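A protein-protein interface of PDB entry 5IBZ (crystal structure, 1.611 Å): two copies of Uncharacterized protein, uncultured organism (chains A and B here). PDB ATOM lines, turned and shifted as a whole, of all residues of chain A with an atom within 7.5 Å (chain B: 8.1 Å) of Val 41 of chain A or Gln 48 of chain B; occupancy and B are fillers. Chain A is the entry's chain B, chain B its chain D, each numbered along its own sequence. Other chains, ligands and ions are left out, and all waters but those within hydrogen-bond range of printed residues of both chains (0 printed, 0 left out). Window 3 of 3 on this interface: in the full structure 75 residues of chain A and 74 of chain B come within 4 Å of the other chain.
OG1 of Thr 49 of chain B sits at hydrogen-bond distance from N of Lys 51 of chain B (3.2 Å). The backbone NH (N) of Val 322 of chain B is in hydrogen-bond range of the backbone carbonyl oxygen (O) of Phe 301 of chain B. The chain-end carboxylate (OXT) of Lys 323 of chain B sits at hydrogen-bond distance from the backbone NH (N) of Gln 48 of chain B (3.0 Å). The backbone carbonyl oxygen of Val 41 of chain A lies within hydrogen-bond range of the guanidinium group of Arg 45 of chain A (3.1 Å). O of Arg 45 of chain B sits at hydrogen-bond distance from NE2 of Gln 48 of chain B, at 2.9 Å. N of Gly 50 of chain B is in hydrogen-bond range of O of Lys 323 of chain B (2.8 Å).
Along chain B the printed residues that touch a printed residue of chain A span positions 44 to 322. Among the printed residues, 13 pairs touch across the chains. Among the printed residues, no Asp or Glu carboxylate lies within 4 Å of a Lys or Arg side-chain nitrogen of the other chain.
The guanidinium group of Arg 45 of chain A sits close to the guanidinium group of Arg 45 of chain B (3.1 Å). O of Ala 44 of chain B sits at hydrogen-bond distance from NH1 of Arg 45 of chain A (2.7 Å). The backbone carbonyl oxygen (O) of Ala 44 of chain A is in hydrogen-bond range of the guanidinium group (NH2) of Arg 45 of chain B, 2.7 Å away. NH2 of Arg 45 of chain A is in hydrogen-bond range of O of Ile 47 of chain B, 3.0 Å away.
Ala 44 of chain A touches Arg 45 of chain B, and with the chains exchanged Arg 45 of chain A touches Ala 44 of chain B. Arg 45 of chain A touches its own counterpart, Arg 45 of chain B. Phe 301 of chain A touches its own counterpart, Phe 301 of chain B. 6 positions are printed for both chains.
Among the printed residues, pairs that only touch across the chains: Pro 37 of chain A with Thr 49 of chain B, Pro 37 of chain A with Gly 50 of chain B, Ile 40 of chain A with Gly 50 of chain B, Val 41 of chain A with Gln 48 of chain B, Val 41 of chain A with Thr 49 of chain B, Val 41 of chain A with Gly 50 of chain B, Ala 44 of chain A with Ile 47 of chain B, Leu 156 of chain A with Val 322 of chain B and Phe 301 of chain A with Phe 301 of chain B.
Of the printed residues of chain B, Val 41 of chain A touches Gln 48, Thr 49 and Gly 50. Of the printed residues of chain A, Gln 48 of chain B touches Val 41 (3.6 Å). Of the printed residues of chain B, Phe 301 of chain A touches Phe 301. Of the printed residues of chain A, Ala 44 of chain B touches Arg 45 (2.7 Å). Of the printed residues of chain A, Arg 45 of chain B touches Ala 44 (2.7 Å) and Arg 45 (3.1 Å). Printed residues of chain B within 4 Å of Ile 40 of chain A: Gly 50. Of the printed residues of chain A, Val 322 of chain B touches Leu 156 (3.8 Å). Lys 51 of chain B touches none of the printed residues of chain A. Arg 39 of chain A touches none of the printed residues of chain B. The nearest printed residue of chain A that does not touch Ile 47 of chain B is Val 41 of chain A (4.1 Å).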
ATOM      1  N   THR A  36      14.765  25.428  -2.965  1.00  0.00           N
ATOM      2  CA  THR A  36      15.606  26.614  -2.923  1.00  0.00           C
ATOM      3  C   THR A  36      16.132  26.887  -4.317  1.00  0.00           C
ATOM      4  O   THR A  36      16.124  25.995  -5.167  1.00  0.00           O
ATOM      5  CB  THR A  36      16.799  26.410  -1.994  1.00  0.00           C
ATOM      6  OG1 THR A  36      17.617  25.365  -2.525  1.00  0.00           O
ATOM      7  CG2 THR A  36      16.331  26.038  -0.581  1.00  0.00           C
ATOM      8  N   PRO A  37      16.624  28.109  -4.558  1.00  0.00           N
ATOM      9  CA  PRO A  37      17.210  28.373  -5.875  1.00  0.00           C
ATOM     10  C   PRO A  37      18.298  27.373  -6.256  1.00  0.00           C
ATOM     11  O   PRO A  37      18.331  26.901  -7.390  1.00  0.00           O
ATOM     12  CB  PRO A  37      17.770  29.801  -5.722  1.00  0.00           C
ATOM     13  CG  PRO A  37      16.856  30.419  -4.720  1.00  0.00           C
ATOM     14  CD  PRO A  37      16.528  29.324  -3.738  1.00  0.00           C
ATOM     15  N   GLU A  38      19.185  27.012  -5.334  1.00  0.00           N
ATOM     16  CA  GLU A  38      20.219  26.033  -5.670  1.00  0.00           C
ATOM     17  C   GLU A  38      19.641  24.669  -6.040  1.00  0.00           C
ATOM     18  O   GLU A  38      20.143  23.998  -6.940  1.00  0.00           O
ATOM     19  CB  GLU A  38      21.214  25.873  -4.524  1.00  0.00           C
ATOM     20  CG  GLU A  38      22.588  25.353  -5.010  1.00  0.00           C
ATOM     21  CD  GLU A  38      23.334  26.345  -5.922  1.00  0.00           C
ATOM     22  OE1 GLU A  38      23.673  27.447  -5.454  1.00  0.00           O
ATOM     23  OE2 GLU A  38      23.588  26.033  -7.107  1.00  0.00           O
ATOM     24  N   ARG A  39      18.564  24.253  -5.389  1.00  0.00           N
ATOM     25  CA  ARG A  39      17.952  22.984  -5.734  1.00  0.00           C
ATOM     26  C   ARG A  39      17.278  23.024  -7.097  1.00  0.00           C
ATOM     27  O   ARG A  39      17.255  22.013  -7.782  1.00  0.00           O
ATOM     28  CB  ARG A  39      16.996  22.561  -4.624  1.00  0.00           C
ATOM     29  CG  ARG A  39      17.842  22.181  -3.409  1.00  0.00           C
ATOM     30  CD  ARG A  39      17.104  22.078  -2.111  1.00  0.00           C
ATOM     31  NE  ARG A  39      18.054  21.702  -1.066  1.00  0.00           N
ATOM     32  CZ  ARG A  39      17.824  21.838   0.236  1.00  0.00           C
ATOM     33  NH1 ARG A  39      16.675  22.322   0.660  1.00  0.00           N
ATOM     34  NH2 ARG A  39      18.760  21.483   1.122  1.00  0.00           N
ATOM     35  N   ILE A  40      16.727  24.177  -7.477  1.00  0.00           N
ATOM     36  CA  ILE A  40      16.171  24.362  -8.820  1.00  0.00           C
ATOM     37  C   ILE A  40      17.270  24.320  -9.894  1.00  0.00           C
ATOM     38  O   ILE A  40      17.098  23.698 -10.931  1.00  0.00           O
ATOM     39  CB  ILE A  40      15.389  25.675  -8.905  1.00  0.00           C
ATOM     40  CG1 ILE A  40      14.184  25.590  -7.979  1.00  0.00           C
ATOM     41  CG2 ILE A  40      14.944  25.939 -10.343  1.00  0.00           C
ATOM     42  CD1 ILE A  40      13.463  26.924  -7.781  1.00  0.00           C
ATOM     43  N   VAL A  41      18.396  24.959  -9.620  1.00  0.00           N
ATOM     44  CA  VAL A  41      19.525  24.918 -10.557  1.00  0.00           C
ATOM     45  C   VAL A  41      19.994  23.474 -10.724  1.00  0.00           C
ATOM     46  O   VAL A  41      20.254  23.019 -11.848  1.00  0.00           O
ATOM     47  CB  VAL A  41      20.662  25.821 -10.070  1.00  0.00           C
ATOM     48  CG1 VAL A  41      21.925  25.621 -10.922  1.00  0.00           C
ATOM     49  CG2 VAL A  41      20.220  27.260 -10.107  1.00  0.00           C
ATOM     50  N   ALA A  42      20.132  22.741  -9.624  1.00  0.00           N
ATOM     51  CA  ALA A  42      20.516  21.335  -9.718  1.00  0.00           C
ATOM     52  C   ALA A  42      19.520  20.502 -10.539  1.00  0.00           C
ATOM     53  O   ALA A  42      19.917  19.673 -11.372  1.00  0.00           O
ATOM     54  CB  ALA A  42      20.673  20.727  -8.308  1.00  0.00           C
ATOM     55  N   ALA A  43      18.225  20.727 -10.332  1.00  0.00           N
ATOM     56  CA  ALA A  43      17.203  20.005 -11.061  1.00  0.00           C
ATOM     57  C   ALA A  43      17.297  20.298 -12.557  1.00  0.00           C
ATOM     58  O   ALA A  43      17.132  19.403 -13.395  1.00  0.00           O
ATOM     59  CB  ALA A  43      15.823  20.375 -10.526  1.00  0.00           C
ATOM     60  N   ALA A  44      17.567  21.553 -12.901  1.00  0.00           N
ATOM     61  CA  ALA A  44      17.691  21.939 -14.304  1.00  0.00           C
ATOM     62  C   ALA A  44      18.803  21.187 -15.014  1.00  0.00           C
ATOM     63  O   ALA A  44      18.737  20.973 -16.234  1.00  0.00           O
ATOM     64  CB  ALA A  44      17.926  23.424 -14.432  1.00  0.00           C
ATOM     65  N   ARG A  45      19.854  20.799 -14.292  1.00  0.00           N
ATOM     66  CA  ARG A  45      20.963  20.070 -14.908  1.00  0.00           C
ATOM     67  C   ARG A  45      20.537  18.656 -15.330  1.00  0.00           C
ATOM     68  O   ARG A  45      21.241  17.976 -16.092  1.00  0.00           O
ATOM     69  CB  ARG A  45      22.160  20.005 -13.948  1.00  0.00           C
ATOM     70  CG  ARG A  45      22.750  21.364 -13.560  1.00  0.00           C
ATOM     71  CD  ARG A  45      23.388  22.132 -14.731  1.00  0.00           C
ATOM     72  NE  ARG A  45      22.448  22.790 -15.632  1.00  0.00           N
ATOM     73  CZ  ARG A  45      21.740  23.884 -15.367  1.00  0.00           C
ATOM     74  NH1 ARG A  45      20.941  24.365 -16.300  1.00  0.00           N
ATOM     75  NH2 ARG A  45      21.782  24.480 -14.178  1.00  0.00           N
ATOM     76  N   LEU A  46      19.386  18.209 -14.838  1.00  0.00           N
ATOM     77  CA  LEU A  46      18.852  16.902 -15.255  1.00  0.00           C
ATOM     78  C   LEU A  46      18.156  16.953 -16.618  1.00  0.00           C
ATOM     79  O   LEU A  46      17.775  15.906 -17.160  1.00  0.00           O
ATOM     80  CB  LEU A  46      17.866  16.358 -14.219  1.00  0.00           C
ATOM     81  CG  LEU A  46      18.456  16.191 -12.832  1.00  0.00           C
ATOM     82  CD1 LEU A  46      17.375  15.676 -11.881  1.00  0.00           C
ATOM     83  CD2 LEU A  46      19.666  15.276 -12.855  1.00  0.00           C
ATOM     84  N   LEU A 156       8.403  23.665  -8.770  1.00  0.00           N
ATOM     85  CA  LEU A 156       9.216  23.585  -9.949  1.00  0.00           C
ATOM     86  C   LEU A 156      10.634  23.333  -9.442  1.00  0.00           C
ATOM     87  O   LEU A 156      11.236  24.200  -8.803  1.00  0.00           O
ATOM     88  CB  LEU A 156       9.054  24.863 -10.762  1.00  0.00           C
ATOM     89  CG  LEU A 156       9.840  24.960 -12.054  1.00  0.00           C
ATOM     90  CD1 LEU A 156       9.049  25.741 -13.096  1.00  0.00           C
ATOM     91  CD2 LEU A 156      11.191  25.599 -11.782  1.00  0.00           C
ATOM     92  N   GLY A 157      11.143  22.124  -9.681  1.00  0.00           N
ATOM     93  CA  GLY A 157      12.364  21.667  -9.050  1.00  0.00           C
ATOM     94  C   GLY A 157      12.584  20.220  -9.395  1.00  0.00           C
ATOM     95  O   GLY A 157      12.204  19.765 -10.486  1.00  0.00           O
ATOM     96  N   PHE A 301      13.603  16.977 -13.933  1.00  0.00           N
ATOM     97  CA  PHE A 301      13.096  18.314 -13.643  1.00  0.00           C
ATOM     98  C   PHE A 301      11.580  18.248 -13.735  1.00  0.00           C
ATOM     99  O   PHE A 301      11.034  17.695 -14.683  1.00  0.00           O
ATOM    100  CB  PHE A 301      13.684  19.352 -14.608  1.00  0.00           C
ATOM    101  CG  PHE A 301      13.232  20.766 -14.365  1.00  0.00           C
ATOM    102  CD1 PHE A 301      12.062  21.249 -14.944  1.00  0.00           C
ATOM    103  CD2 PHE A 301      13.997  21.608 -13.589  1.00  0.00           C
ATOM    104  CE1 PHE A 301      11.670  22.573 -14.735  1.00  0.00           C
ATOM    105  CE2 PHE A 301      13.599  22.926 -13.361  1.00  0.00           C
ATOM    106  CZ  PHE A 301      12.441  23.401 -13.948  1.00  0.00           C
ATOM    107  N   ALA B  42      18.617  23.431 -24.517  1.00  0.00           N
ATOM    108  CA  ALA B  42      19.272  24.743 -24.562  1.00  0.00           C
ATOM    109  C   ALA B  42      18.629  25.710 -23.579  1.00  0.00           C
ATOM    110  O   ALA B  42      19.317  26.456 -22.878  1.00  0.00           O
ATOM    111  CB  ALA B  42      19.228  25.314 -25.978  1.00  0.00           C
ATOM    112  N   ALA B  43      17.303  25.714 -23.521  1.00  0.00           N
ATOM    113  CA  ALA B  43      16.607  26.620 -22.617  1.00  0.00           C
ATOM    114  C   ALA B  43      16.969  26.319 -21.170  1.00  0.00           C
ATOM    115  O   ALA B  43      17.139  27.225 -20.364  1.00  0.00           O
ATOM    116  CB  ALA B  43      15.107  26.521 -22.819  1.00  0.00           C
ATOM    117  N   ALA B  44      17.087  25.036 -20.840  1.00  0.00           N
ATOM    118  CA  ALA B  44      17.392  24.642 -19.470  1.00  0.00           C
ATOM    119  C   ALA B  44      18.745  25.180 -19.012  1.00  0.00           C
ATOM    120  O   ALA B  44      18.943  25.406 -17.817  1.00  0.00           O
ATOM    121  CB  ALA B  44      17.349  23.128 -19.331  1.00  0.00           C
ATOM    122  N   ARG B  45      19.688  25.395 -19.932  1.00  0.00           N
ATOM    123  CA  ARG B  45      20.980  25.928 -19.544  1.00  0.00           C
ATOM    124  C   ARG B  45      20.906  27.382 -19.076  1.00  0.00           C
ATOM    125  O   ARG B  45      21.862  27.892 -18.473  1.00  0.00           O
ATOM    126  CB  ARG B  45      21.979  25.798 -20.699  1.00  0.00           C
ATOM    127  CG  ARG B  45      22.233  24.346 -21.150  1.00  0.00           C
ATOM    128  CD  ARG B  45      22.989  23.540 -20.112  1.00  0.00           C
ATOM    129  NE  ARG B  45      22.143  23.088 -19.007  1.00  0.00           N
ATOM    130  CZ  ARG B  45      21.204  22.149 -19.090  1.00  0.00           C
ATOM    131  NH1 ARG B  45      20.946  21.524 -20.241  1.00  0.00           N
ATOM    132  NH2 ARG B  45      20.502  21.854 -18.012  1.00  0.00           N
ATOM    133  N   LEU B  46      19.782  28.050 -19.336  1.00  0.00           N
ATOM    134  CA  LEU B  46      19.573  29.421 -18.869  1.00  0.00           C
ATOM    135  C   LEU B  46      19.215  29.486 -17.383  1.00  0.00           C
ATOM    136  O   LEU B  46      19.162  30.576 -16.790  1.00  0.00           O
ATOM    137  CB  LEU B  46      18.474  30.102 -19.677  1.00  0.00           C
ATOM    138  CG  LEU B  46      18.795  30.190 -21.168  1.00  0.00           C
ATOM    139  CD1 LEU B  46      17.640  30.847 -21.887  1.00  0.00           C
ATOM    140  CD2 LEU B  46      20.079  30.937 -21.416  1.00  0.00           C
ATOM    141  N   ILE B  47      18.949  28.335 -16.789  1.00  0.00           N
ATOM    142  CA  ILE B  47      18.648  28.261 -15.369  1.00  0.00           C
ATOM    143  C   ILE B  47      19.972  28.257 -14.605  1.00  0.00           C
ATOM    144  O   ILE B  47      20.606  27.217 -14.427  1.00  0.00           O
ATOM    145  CB  ILE B  47      17.790  27.032 -15.017  1.00  0.00           C
ATOM    146  CG1 ILE B  47      16.446  27.120 -15.762  1.00  0.00           C
ATOM    147  CG2 ILE B  47      17.539  27.001 -13.526  1.00  0.00           C
ATOM    148  CD1 ILE B  47      15.533  25.904 -15.591  1.00  0.00           C
ATOM    149  N   GLN B  48      20.378  29.445 -14.168  1.00  0.00           N
ATOM    150  CA  GLN B  48      21.675  29.564 -13.501  1.00  0.00           C
ATOM    151  C   GLN B  48      21.568  30.189 -12.110  1.00  0.00           C
ATOM    152  O   GLN B  48      22.426  29.901 -11.252  1.00  0.00           O
ATOM    153  CB  GLN B  48      22.664  30.361 -14.361  1.00  0.00           C
ATOM    154  CG  GLN B  48      23.091  29.659 -15.659  1.00  0.00           C
ATOM    155  CD  GLN B  48      23.895  28.382 -15.433  1.00  0.00           C
ATOM    156  OE1 GLN B  48      24.692  28.284 -14.491  1.00  0.00           O
ATOM    157  NE2 GLN B  48      23.703  27.401 -16.312  1.00  0.00           N
ATOM    158  N   THR B  49      20.539  30.995 -11.856  1.00  0.00           N
ATOM    159  CA  THR B  49      20.292  31.566 -10.517  1.00  0.00           C
ATOM    160  C   THR B  49      19.246  30.792  -9.722  1.00  0.00           C
ATOM    161  O   THR B  49      19.304  30.732  -8.497  1.00  0.00           O
ATOM    162  CB  THR B  49      19.837  33.034 -10.582  1.00  0.00           C
ATOM    163  OG1 THR B  49      18.528  33.123 -11.160  1.00  0.00           O
ATOM    164  CG2 THR B  49      20.797  33.854 -11.413  1.00  0.00           C
ATOM    165  N   GLY B  50      18.283  30.200 -10.415  1.00  0.00           N
ATOM    166  CA  GLY B  50      17.207  29.490  -9.765  1.00  0.00           C
ATOM    167  C   GLY B  50      16.092  30.400  -9.293  1.00  0.00           C
ATOM    168  O   GLY B  50      15.202  29.957  -8.557  1.00  0.00           O
ATOM    169  N   LYS B  51      16.111  31.658  -9.721  1.00  0.00           N
ATOM    170  CA  LYS B  51      15.032  32.595  -9.418  1.00  0.00           C
ATOM    171  C   LYS B  51      13.848  32.247 -10.291  1.00  0.00           C
ATOM    172  O   LYS B  51      14.034  31.911 -11.454  1.00  0.00           O
ATOM    173  CB  LYS B  51      15.432  34.052  -9.695  1.00  0.00           C
ATOM    174  CG  LYS B  51      16.566  34.639  -8.874  1.00  0.00           C
ATOM    175  CD  LYS B  51      16.843  36.108  -9.333  1.00  0.00           C
ATOM    176  CE  LYS B  51      17.586  36.192 -10.678  1.00  0.00           C
ATOM    177  NZ  LYS B  51      17.783  37.599 -11.169  1.00  0.00           N
ATOM    178  N   ARG B 297      19.424  40.232 -18.328  1.00  0.00           N
ATOM    179  CA  ARG B 297      19.068  38.967 -18.958  1.00  0.00           C
ATOM    180  C   ARG B 297      17.574  38.922 -19.288  1.00  0.00           C
ATOM    181  O   ARG B 297      16.735  38.899 -18.390  1.00  0.00           O
ATOM    182  CB  ARG B 297      19.429  37.784 -18.048  1.00  0.00           C
ATOM    183  CG  ARG B 297      20.904  37.654 -17.701  1.00  0.00           C
ATOM    184  CD  ARG B 297      21.130  36.484 -16.719  1.00  0.00           C
ATOM    185  NE  ARG B 297      20.591  35.236 -17.264  1.00  0.00           N
ATOM    186  CZ  ARG B 297      20.163  34.193 -16.541  1.00  0.00           C
ATOM    187  NH1 ARG B 297      20.217  34.202 -15.218  1.00  0.00           N
ATOM    188  NH2 ARG B 297      19.684  33.119 -17.154  1.00  0.00           N
ATOM    189  N   PHE B 301      14.287  30.273 -19.129  1.00  0.00           N
ATOM    190  CA  PHE B 301      13.497  29.058 -19.264  1.00  0.00           C
ATOM    191  C   PHE B 301      12.072  29.391 -18.892  1.00  0.00           C
ATOM    192  O   PHE B 301      11.827  30.040 -17.879  1.00  0.00           O
ATOM    193  CB  PHE B 301      14.054  27.956 -18.369  1.00  0.00           C
ATOM    194  CG  PHE B 301      13.298  26.662 -18.403  1.00  0.00           C
ATOM    195  CD1 PHE B 301      12.237  26.438 -17.539  1.00  0.00           C
ATOM    196  CD2 PHE B 301      13.694  25.651 -19.243  1.00  0.00           C
ATOM    197  CE1 PHE B 301      11.556  25.228 -17.543  1.00  0.00           C
ATOM    198  CE2 PHE B 301      13.001  24.435 -19.250  1.00  0.00           C
ATOM    199  CZ  PHE B 301      11.927  24.242 -18.402  1.00  0.00           C
ATOM    200  N   VAL B 322      12.014  31.084 -15.314  1.00  0.00           N
ATOM    201  CA  VAL B 322      13.120  30.647 -14.464  1.00  0.00           C
ATOM    202  C   VAL B 322      14.436  31.148 -15.020  1.00  0.00           C
ATOM    203  O   VAL B 322      14.738  30.980 -16.205  1.00  0.00           O
ATOM    204  CB  VAL B 322      13.180  29.109 -14.357  1.00  0.00           C
ATOM    205  CG1 VAL B 322      14.117  28.695 -13.243  1.00  0.00           C
ATOM    206  CG2 VAL B 322      11.794  28.508 -14.151  1.00  0.00           C
ATOM    207  N   LYS B 323      15.228  31.772 -14.165  1.00  0.00           N
ATOM    208  CA  LYS B 323      16.522  32.293 -14.579  1.00  0.00           C
ATOM    209  C   LYS B 323      17.631  31.647 -13.778  1.00  0.00           C
ATOM    210  O   LYS B 323      17.356  30.741 -13.001  1.00  0.00           O
ATOM    211  CB  LYS B 323      16.547  33.818 -14.431  1.00  0.00           C
ATOM    212  CG  LYS B 323      15.674  34.496 -15.483  1.00  0.00           C
ATOM    213  CD  LYS B 323      15.453  35.991 -15.225  1.00  0.00           C
ATOM    214  CE  LYS B 323      16.640  36.821 -15.664  1.00  0.00           C
ATOM    215  NZ  LYS B 323      16.368  38.253 -15.428  1.00  0.00           N
ATOM    216  OXT LYS B 323      18.801  32.018 -13.907  1.00  0.00           O
